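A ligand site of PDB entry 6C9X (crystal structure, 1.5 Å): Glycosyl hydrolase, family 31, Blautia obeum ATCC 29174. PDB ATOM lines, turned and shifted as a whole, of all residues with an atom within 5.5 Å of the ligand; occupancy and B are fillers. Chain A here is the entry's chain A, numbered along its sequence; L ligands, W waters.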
ATOM      1  N   ASP A  76     -21.230 -32.649   5.002  1.00  0.00           N
ATOM      2  CA  ASP A  76     -20.376 -31.546   4.614  1.00  0.00           C
ATOM      3  C   ASP A  76     -18.921 -31.987   4.761  1.00  0.00           C
ATOM      4  O   ASP A  76     -18.367 -31.975   5.865  1.00  0.00           O
ATOM      5  CB  ASP A  76     -20.663 -30.318   5.502  1.00  0.00           C
ATOM      6  CG  ASP A  76     -19.820 -29.121   5.140  1.00  0.00           C
ATOM      7  OD1 ASP A  76     -18.868 -29.251   4.338  1.00  0.00           O
ATOM      8  OD2 ASP A  76     -20.103 -28.027   5.678  1.00  0.00           O
ATOM      9  N   PRO A  78     -15.340 -31.180   2.706  1.00  0.00           N
ATOM     10  CA  PRO A  78     -14.704 -30.392   1.639  1.00  0.00           C
ATOM     11  C   PRO A  78     -13.456 -31.047   1.057  1.00  0.00           C
ATOM     12  O   PRO A  78     -12.701 -30.394   0.324  1.00  0.00           O
ATOM     13  CB  PRO A  78     -14.325 -29.105   2.363  1.00  0.00           C
ATOM     14  CG  PRO A  78     -13.973 -29.582   3.761  1.00  0.00           C
ATOM     15  CD  PRO A  78     -15.004 -30.664   4.048  1.00  0.00           C
ATOM     16  N   TRP A 172     -16.109 -16.664  -2.372  1.00  0.00           N
ATOM     17  CA  TRP A 172     -16.328 -16.448  -0.957  1.00  0.00           C
ATOM     18  C   TRP A 172     -15.433 -15.286  -0.546  1.00  0.00           C
ATOM     19  O   TRP A 172     -14.220 -15.444  -0.382  1.00  0.00           O
ATOM     20  CB  TRP A 172     -15.977 -17.731  -0.209  1.00  0.00           C
ATOM     21  CG  TRP A 172     -16.173 -17.679   1.273  1.00  0.00           C
ATOM     22  CD1 TRP A 172     -16.806 -16.705   1.998  1.00  0.00           C
ATOM     23  CD2 TRP A 172     -15.724 -18.661   2.222  1.00  0.00           C
ATOM     24  NE1 TRP A 172     -16.782 -17.018   3.335  1.00  0.00           N
ATOM     25  CE2 TRP A 172     -16.130 -18.210   3.501  1.00  0.00           C
ATOM     26  CE3 TRP A 172     -15.035 -19.863   2.116  1.00  0.00           C
ATOM     27  CZ2 TRP A 172     -15.846 -18.937   4.671  1.00  0.00           C
ATOM     28  CZ3 TRP A 172     -14.756 -20.583   3.275  1.00  0.00           C
ATOM     29  CH2 TRP A 172     -15.157 -20.111   4.529  1.00  0.00           C
ATOM     30  N   ASP A 200     -22.003 -14.441  -2.131  1.00  0.00           N
ATOM     31  CA  ASP A 200     -21.779 -15.378  -1.035  1.00  0.00           C
ATOM     32  C   ASP A 200     -22.105 -14.688   0.292  1.00  0.00           C
ATOM     33  O   ASP A 200     -22.505 -13.528   0.301  1.00  0.00           O
ATOM     34  CB  ASP A 200     -20.322 -15.871  -1.098  1.00  0.00           C
ATOM     35  CG  ASP A 200     -20.155 -17.273  -0.560  1.00  0.00           C
ATOM     36  OD1 ASP A 200     -20.917 -17.674   0.347  1.00  0.00           O
ATOM     37  OD2 ASP A 200     -19.241 -17.988  -1.042  1.00  0.00           O
ATOM     38  N   ILE A 201     -21.906 -15.393   1.399  1.00  0.00           N
ATOM     39  CA  ILE A 201     -22.525 -15.034   2.693  1.00  0.00           C
ATOM     40  C   ILE A 201     -22.255 -13.627   3.230  1.00  0.00           C
ATOM     41  O   ILE A 201     -22.978 -13.136   4.093  1.00  0.00           O
ATOM     42  CB  ILE A 201     -22.155 -16.075   3.793  1.00  0.00           C
ATOM     43  CG1 ILE A 201     -20.637 -16.247   3.888  1.00  0.00           C
ATOM     44  CG2 ILE A 201     -22.849 -17.410   3.522  1.00  0.00           C
ATOM     45  CD1 ILE A 201     -20.212 -17.244   4.981  1.00  0.00           C
ATOM     46  N   ILE A 237     -26.780 -16.385  -2.006  1.00  0.00           N
ATOM     47  CA  ILE A 237     -26.819 -17.632  -1.252  1.00  0.00           C
ATOM     48  C   ILE A 237     -27.813 -17.497  -0.090  1.00  0.00           C
ATOM     49  O   ILE A 237     -28.020 -16.407   0.455  1.00  0.00           O
ATOM     50  CB  ILE A 237     -25.387 -17.959  -0.723  1.00  0.00           C
ATOM     51  CG1 ILE A 237     -25.287 -19.406  -0.217  1.00  0.00           C
ATOM     52  CG2 ILE A 237     -24.933 -16.969   0.365  1.00  0.00           C
ATOM     53  CD1 ILE A 237     -23.845 -19.829   0.045  1.00  0.00           C
ATOM     54  N   ASP A 239     -28.681 -19.842   3.489  1.00  0.00           N
ATOM     55  CA  ASP A 239     -28.224 -20.942   4.344  1.00  0.00           C
ATOM     56  C   ASP A 239     -29.349 -21.632   5.100  1.00  0.00           C
ATOM     57  O   ASP A 239     -30.386 -21.039   5.386  1.00  0.00           O
ATOM     58  CB  ASP A 239     -27.199 -20.416   5.367  1.00  0.00           C
ATOM     59  CG  ASP A 239     -25.877 -20.043   4.745  1.00  0.00           C
ATOM     60  OD1 ASP A 239     -25.435 -20.735   3.809  1.00  0.00           O
ATOM     61  OD2 ASP A 239     -25.267 -19.062   5.213  1.00  0.00           O
ATOM     62  N   TRP A 274     -22.302 -20.124  10.273  1.00  0.00           N
ATOM     63  CA  TRP A 274     -21.703 -18.790  10.071  1.00  0.00           C
ATOM     64  C   TRP A 274     -22.106 -17.670  11.044  1.00  0.00           C
ATOM     65  O   TRP A 274     -21.248 -16.878  11.462  1.00  0.00           O
ATOM     66  CB  TRP A 274     -21.869 -18.334   8.619  1.00  0.00           C
ATOM     67  CG  TRP A 274     -21.456 -19.366   7.623  1.00  0.00           C
ATOM     68  CD1 TRP A 274     -22.271 -20.011   6.716  1.00  0.00           C
ATOM     69  CD2 TRP A 274     -20.152 -19.902   7.435  1.00  0.00           C
ATOM     70  NE1 TRP A 274     -21.548 -20.908   5.989  1.00  0.00           N
ATOM     71  CE2 TRP A 274     -20.242 -20.870   6.407  1.00  0.00           C
ATOM     72  CE3 TRP A 274     -18.911 -19.684   8.047  1.00  0.00           C
ATOM     73  CZ2 TRP A 274     -19.132 -21.597   5.969  1.00  0.00           C
ATOM     74  CZ3 TRP A 274     -17.810 -20.407   7.607  1.00  0.00           C
ATOM     75  CH2 TRP A 274     -17.933 -21.350   6.573  1.00  0.00           C
ATOM     76  N   TRP A 308     -28.927 -19.800  -4.546  1.00  0.00           N
ATOM     77  CA  TRP A 308     -28.309 -21.090  -4.246  1.00  0.00           C
ATOM     78  C   TRP A 308     -28.461 -21.406  -2.767  1.00  0.00           C
ATOM     79  O   TRP A 308     -28.232 -20.544  -1.921  1.00  0.00           O
ATOM     80  CB  TRP A 308     -26.853 -21.204  -4.772  1.00  0.00           C
ATOM     81  CG  TRP A 308     -25.881 -20.079  -4.454  1.00  0.00           C
ATOM     82  CD1 TRP A 308     -26.074 -18.738  -4.625  1.00  0.00           C
ATOM     83  CD2 TRP A 308     -24.523 -20.229  -3.987  1.00  0.00           C
ATOM     84  NE1 TRP A 308     -24.938 -18.045  -4.272  1.00  0.00           N
ATOM     85  CE2 TRP A 308     -23.974 -18.937  -3.872  1.00  0.00           C
ATOM     86  CE3 TRP A 308     -23.735 -21.329  -3.641  1.00  0.00           C
ATOM     87  CZ2 TRP A 308     -22.665 -18.719  -3.425  1.00  0.00           C
ATOM     88  CZ3 TRP A 308     -22.438 -21.115  -3.201  1.00  0.00           C
ATOM     89  CH2 TRP A 308     -21.917 -19.821  -3.097  1.00  0.00           C
ATOM     90  N   ASP A 310     -27.421 -23.512   0.587  1.00  0.00           N
ATOM     91  CA  ASP A 310     -26.164 -24.081   1.085  1.00  0.00           C
ATOM     92  C   ASP A 310     -26.258 -24.540   2.539  1.00  0.00           C
ATOM     93  O   ASP A 310     -27.219 -24.203   3.248  1.00  0.00           O
ATOM     94  CB  ASP A 310     -25.048 -23.047   0.943  1.00  0.00           C
ATOM     95  CG  ASP A 310     -23.674 -23.606   1.198  1.00  0.00           C
ATOM     96  OD1 ASP A 310     -23.458 -24.814   0.923  1.00  0.00           O
ATOM     97  OD2 ASP A 310     -22.810 -22.830   1.646  1.00  0.00           O
ATOM     98  N   MET A 311     -25.260 -25.315   2.960  1.00  0.00           N
ATOM     99  CA  MET A 311     -25.106 -25.792   4.342  1.00  0.00           C
ATOM    100  C   MET A 311     -26.307 -26.634   4.764  1.00  0.00           C
ATOM    101  O   MET A 311     -26.635 -26.720   5.940  1.00  0.00           O
ATOM    102  CB  MET A 311     -24.883 -24.631   5.311  1.00  0.00           C
ATOM    103  CG  MET A 311     -23.808 -23.650   4.871  1.00  0.00           C
ATOM    104  SD  MET A 311     -22.171 -24.376   4.725  1.00  0.00           S
ATOM    105  CE  MET A 311     -21.675 -24.545   6.449  1.00  0.00           C
ATOM    106  N   PHE A 317     -21.385 -26.717  12.820  1.00  0.00           N
ATOM    107  CA  PHE A 317     -20.003 -26.521  13.291  1.00  0.00           C
ATOM    108  C   PHE A 317     -19.858 -27.116  14.686  1.00  0.00           C
ATOM    109  O   PHE A 317     -18.814 -27.669  15.042  1.00  0.00           O
ATOM    110  CB  PHE A 317     -19.605 -25.033  13.329  1.00  0.00           C
ATOM    111  CG  PHE A 317     -19.565 -24.351  11.973  1.00  0.00           C
ATOM    112  CD1 PHE A 317     -19.697 -25.056  10.777  1.00  0.00           C
ATOM    113  CD2 PHE A 317     -19.392 -22.977  11.911  1.00  0.00           C
ATOM    114  CE1 PHE A 317     -19.665 -24.387   9.551  1.00  0.00           C
ATOM    115  CE2 PHE A 317     -19.361 -22.303  10.697  1.00  0.00           C
ATOM    116  CZ  PHE A 317     -19.496 -23.011   9.511  1.00  0.00           C
ATOM    117  N   ARG A 407     -26.895 -27.570  -2.383  1.00  0.00           N
ATOM    118  CA  ARG A 407     -25.734 -28.417  -2.134  1.00  0.00           C
ATOM    119  C   ARG A 407     -26.169 -29.849  -1.827  1.00  0.00           C
ATOM    120  O   ARG A 407     -25.744 -30.799  -2.494  1.00  0.00           O
ATOM    121  CB  ARG A 407     -24.857 -27.856  -1.014  1.00  0.00           C
ATOM    122  CG  ARG A 407     -23.468 -28.465  -1.054  1.00  0.00           C
ATOM    123  CD  ARG A 407     -22.494 -27.734  -0.141  1.00  0.00           C
ATOM    124  NE  ARG A 407     -22.736 -28.021   1.263  1.00  0.00           N
ATOM    125  CZ  ARG A 407     -21.940 -27.635   2.244  1.00  0.00           C
ATOM    126  NH1 ARG A 407     -22.210 -27.949   3.503  1.00  0.00           N
ATOM    127  NH2 ARG A 407     -20.841 -26.940   1.957  1.00  0.00           N
ATOM    128  N   TRP A 420     -25.012 -28.040  -7.334  1.00  0.00           N
ATOM    129  CA  TRP A 420     -23.607 -27.931  -7.692  1.00  0.00           C
ATOM    130  C   TRP A 420     -22.875 -28.993  -6.878  1.00  0.00           C
ATOM    131  O   TRP A 420     -23.391 -29.455  -5.854  1.00  0.00           O
ATOM    132  CB  TRP A 420     -23.037 -26.520  -7.504  1.00  0.00           C
ATOM    133  CG  TRP A 420     -22.417 -26.163  -6.175  1.00  0.00           C
ATOM    134  CD1 TRP A 420     -21.082 -26.093  -5.893  1.00  0.00           C
ATOM    135  CD2 TRP A 420     -23.097 -25.726  -4.983  1.00  0.00           C
ATOM    136  NE1 TRP A 420     -20.894 -25.684  -4.593  1.00  0.00           N
ATOM    137  CE2 TRP A 420     -22.116 -25.436  -4.013  1.00  0.00           C
ATOM    138  CE3 TRP A 420     -24.447 -25.566  -4.647  1.00  0.00           C
ATOM    139  CZ2 TRP A 420     -22.424 -24.999  -2.743  1.00  0.00           C
ATOM    140  CZ3 TRP A 420     -24.763 -25.111  -3.362  1.00  0.00           C
ATOM    141  CH2 TRP A 420     -23.749 -24.841  -2.419  1.00  0.00           C
ATOM    142  N   GLY A 422     -20.456 -29.064  -4.921  1.00  0.00           N
ATOM    143  CA  GLY A 422     -19.926 -28.741  -3.608  1.00  0.00           C
ATOM    144  C   GLY A 422     -18.488 -28.256  -3.619  1.00  0.00           C
ATOM    145  O   GLY A 422     -18.016 -27.701  -4.618  1.00  0.00           O
ATOM    146  N   ASP A 423     -17.800 -28.473  -2.502  1.00  0.00           N
ATOM    147  CA  ASP A 423     -16.446 -27.965  -2.336  1.00  0.00           C
ATOM    148  C   ASP A 423     -15.416 -28.924  -2.886  1.00  0.00           C
ATOM    149  O   ASP A 423     -14.845 -29.730  -2.145  1.00  0.00           O
ATOM    150  CB  ASP A 423     -16.179 -27.683  -0.863  1.00  0.00           C
ATOM    151  CG  ASP A 423     -17.117 -26.632  -0.299  1.00  0.00           C
ATOM    152  OD1 ASP A 423     -17.619 -25.808  -1.096  1.00  0.00           O
ATOM    153  OD2 ASP A 423     -17.359 -26.641   0.927  1.00  0.00           O
ATOM    154  N   ASP A 452     -17.462 -26.372  -9.224  1.00  0.00           N
ATOM    155  CA  ASP A 452     -16.751 -25.103  -9.116  1.00  0.00           C
ATOM    156  C   ASP A 452     -15.550 -25.083 -10.057  1.00  0.00           C
ATOM    157  O   ASP A 452     -14.545 -25.759  -9.828  1.00  0.00           O
ATOM    158  CB  ASP A 452     -16.310 -24.850  -7.671  1.00  0.00           C
ATOM    159  CG  ASP A 452     -17.457 -24.450  -6.757  1.00  0.00           C
ATOM    160  OD1 ASP A 452     -18.613 -24.320  -7.214  1.00  0.00           O
ATOM    161  OD2 ASP A 452     -17.193 -24.243  -5.561  1.00  0.00           O
ATOM    162  N   PHE A 456     -12.765 -25.157  -6.011  1.00  0.00           N
ATOM    163  CA  PHE A 456     -13.146 -24.272  -4.915  1.00  0.00           C
ATOM    164  C   PHE A 456     -11.978 -24.055  -3.960  1.00  0.00           C
ATOM    165  O   PHE A 456     -11.503 -22.920  -3.781  1.00  0.00           O
ATOM    166  CB  PHE A 456     -14.350 -24.864  -4.170  1.00  0.00           C
ATOM    167  CG  PHE A 456     -14.708 -24.151  -2.895  1.00  0.00           C
ATOM    168  CD1 PHE A 456     -15.403 -22.936  -2.912  1.00  0.00           C
ATOM    169  CD2 PHE A 456     -14.391 -24.710  -1.665  1.00  0.00           C
ATOM    170  CE1 PHE A 456     -15.748 -22.300  -1.726  1.00  0.00           C
ATOM    171  CE2 PHE A 456     -14.744 -24.094  -0.478  1.00  0.00           C
ATOM    172  CZ  PHE A 456     -15.423 -22.877  -0.510  1.00  0.00           C
ATOM    173  N   ARG A 479     -19.911 -22.253 -13.639  1.00  0.00           N
ATOM    174  CA  ARG A 479     -19.600 -21.270 -12.614  1.00  0.00           C
ATOM    175  C   ARG A 479     -18.191 -21.435 -12.073  1.00  0.00           C
ATOM    176  O   ARG A 479     -17.821 -22.519 -11.614  1.00  0.00           O
ATOM    177  CB  ARG A 479     -20.590 -21.406 -11.441  1.00  0.00           C
ATOM    178  CG  ARG A 479     -20.306 -20.495 -10.270  1.00  0.00           C
ATOM    179  CD  ARG A 479     -21.315 -20.688  -9.158  1.00  0.00           C
ATOM    180  NE  ARG A 479     -20.962 -21.790  -8.257  1.00  0.00           N
ATOM    181  CZ  ARG A 479     -21.334 -21.838  -6.986  1.00  0.00           C
ATOM    182  NH1 ARG A 479     -22.073 -20.857  -6.476  1.00  0.00           N
ATOM    183  NH2 ARG A 479     -20.979 -22.867  -6.219  1.00  0.00           N
ATOM    184  N   HIS A 481     -16.004 -20.547  -9.080  1.00  0.00           N
ATOM    185  CA  HIS A 481     -16.208 -20.172  -7.673  1.00  0.00           C
ATOM    186  C   HIS A 481     -14.993 -20.626  -6.880  1.00  0.00           C
ATOM    187  O   HIS A 481     -14.358 -21.640  -7.229  1.00  0.00           O
ATOM    188  CB  HIS A 481     -17.506 -20.807  -7.141  1.00  0.00           C
ATOM    189  CG  HIS A 481     -17.812 -20.469  -5.710  1.00  0.00           C
ATOM    190  ND1 HIS A 481     -17.838 -19.168  -5.244  1.00  0.00           N
ATOM    191  CD2 HIS A 481     -18.106 -21.247  -4.643  1.00  0.00           C
ATOM    192  CE1 HIS A 481     -18.136 -19.166  -3.958  1.00  0.00           C
ATOM    193  NE2 HIS A 481     -18.303 -20.420  -3.568  1.00  0.00           N
ATOM    194  N   ALA A 482     -14.657 -19.898  -5.818  1.00  0.00           N
ATOM    195  CA  ALA A 482     -13.450 -20.177  -5.049  1.00  0.00           C
ATOM    196  C   ALA A 482     -13.601 -19.824  -3.581  1.00  0.00           C
ATOM    197  O   ALA A 482     -14.407 -18.959  -3.218  1.00  0.00           O
ATOM    198  CB  ALA A 482     -12.244 -19.460  -5.648  1.00  0.00           C
HETATM  199  C1  LIG L   1     -19.019 -21.284   1.616  1.00  0.00           C
HETATM  200  O1  LIG L   1     -17.633 -21.518   1.805  1.00  0.00           O
HETATM  201  C2  LIG L   1     -19.336 -21.286   0.116  1.00  0.00           C
HETATM  202  O2  LIG L   1     -18.470 -20.435  -0.548  1.00  0.00           O
HETATM  203  C3  LIG L   1     -19.234 -22.683  -0.488  1.00  0.00           C
HETATM  204  O3  LIG L   1     -19.679 -22.647  -1.791  1.00  0.00           O
HETATM  205  C4  LIG L   1     -20.023 -23.705   0.320  1.00  0.00           C
HETATM  206  O4  LIG L   1     -19.969 -24.997  -0.233  1.00  0.00           O
HETATM  207  C5  LIG L   1     -19.598 -23.729   1.756  1.00  0.00           C
HETATM  208  C6  LIG L   1     -19.745 -22.361   2.353  1.00  0.00           C
HETATM  209  C7  LIG L   1     -19.321 -19.955   2.226  1.00  0.00           C
HETATM  210  O5  LIG L   1     -20.660 -19.613   2.117  1.00  0.00           O
HETATM  211  N1  LIG L   1     -18.210 -24.223   1.937  1.00  0.00           N
HETATM  212  C8  LIG L   1     -17.689 -24.246   3.311  1.00  0.00           C
HETATM  213  C9  LIG L   1     -16.264 -24.747   3.311  1.00  0.00           C
HETATM  214  O6  LIG L   1     -15.728 -24.536   4.589  1.00  0.00           O
HETATM  215  C10 LIG L   1     -18.521 -24.971   4.293  1.00  0.00           C
HETATM  216  O7  LIG L   1     -18.868 -26.242   3.884  1.00  0.00           O
HETATM  217  O   HOH W   1     -22.917 -20.838   3.281  1.00  0.00           O
HETATM  218  O   HOH W   2     -18.535 -24.630  -3.382  1.00  0.00           O
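Trp 172 touches the ligand. Ile 201 touches the ligand (CG2 to O5, 3.4 Å). Ile 237 touches the ligand. Trp 274 touches the ligand. Trp 308 touches the ligand. Asp 310 touches the ligand. Met 311 touches the ligand (SD to C10, 3.7 Å). Trp 420 touches the ligand (CZ2 to O4, 3.5 Å). Phe 456 touches the ligand. Hydrophobic or aromatic side chains within 4 Å of the ligand: Trp 172, Ile 201, Ile 237, Trp 274, Trp 308, Met 311, Trp 420, Phe 456 and His 481. Within 4 Å of the ligand: Asp 76, Trp 172, Asp 200, Ile 201, Ile 237, Trp 274, Trp 308, Asp 310, Met 311, Arg 407, Trp 420, Asp 423, Phe 456 and His 481.
OD2 of Asp 423 lies within salt-bridge range of N1 of the ligand (2.8 Å). An oxygen (O7) of the ligand sits at hydrogen-bond distance from the guanidinium group of Arg 407, at 2.8 Å. The side-chain carboxylate of Asp 200 is in hydrogen-bond range of an oxygen (O2) of the ligand, at 2.6 Å. O2 of the ligand sits at hydrogen-bond distance from NE2 of His 481 (3.0 Å). The side-chain carboxylate of Asp 76 lies within hydrogen-bond range of an oxygen (O7) of the ligand, 2.8 Å away.
Water W1 lies within hydrogen-bond range of the side-chain carboxylate of Asp 239, the side-chain carboxylate of Asp 310, an oxygen (O5) of the ligand and the indole nitrogen of Trp 274.
NH1 of Arg 407 sits close to SD of Met 311, 3.8 Å away. The side-chain carboxylate of Asp 76 lies within salt-bridge range of the guanidinium group of Arg 407. NE of Arg 407 is in salt-bridge range of OD1 of Asp 310. The backbone NH of Trp 172 is in hydrogen-bond range of the backbone carbonyl oxygen of Ala 482. The indole nitrogen of Trp 274 lies close to the side-chain sulfur of Met 311, at 3.7 Å. The side-chain carboxylate (OD2) of Asp 423 is in salt-bridge range of the guanidinium group (NH2) of Arg 407 (3.6 Å).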
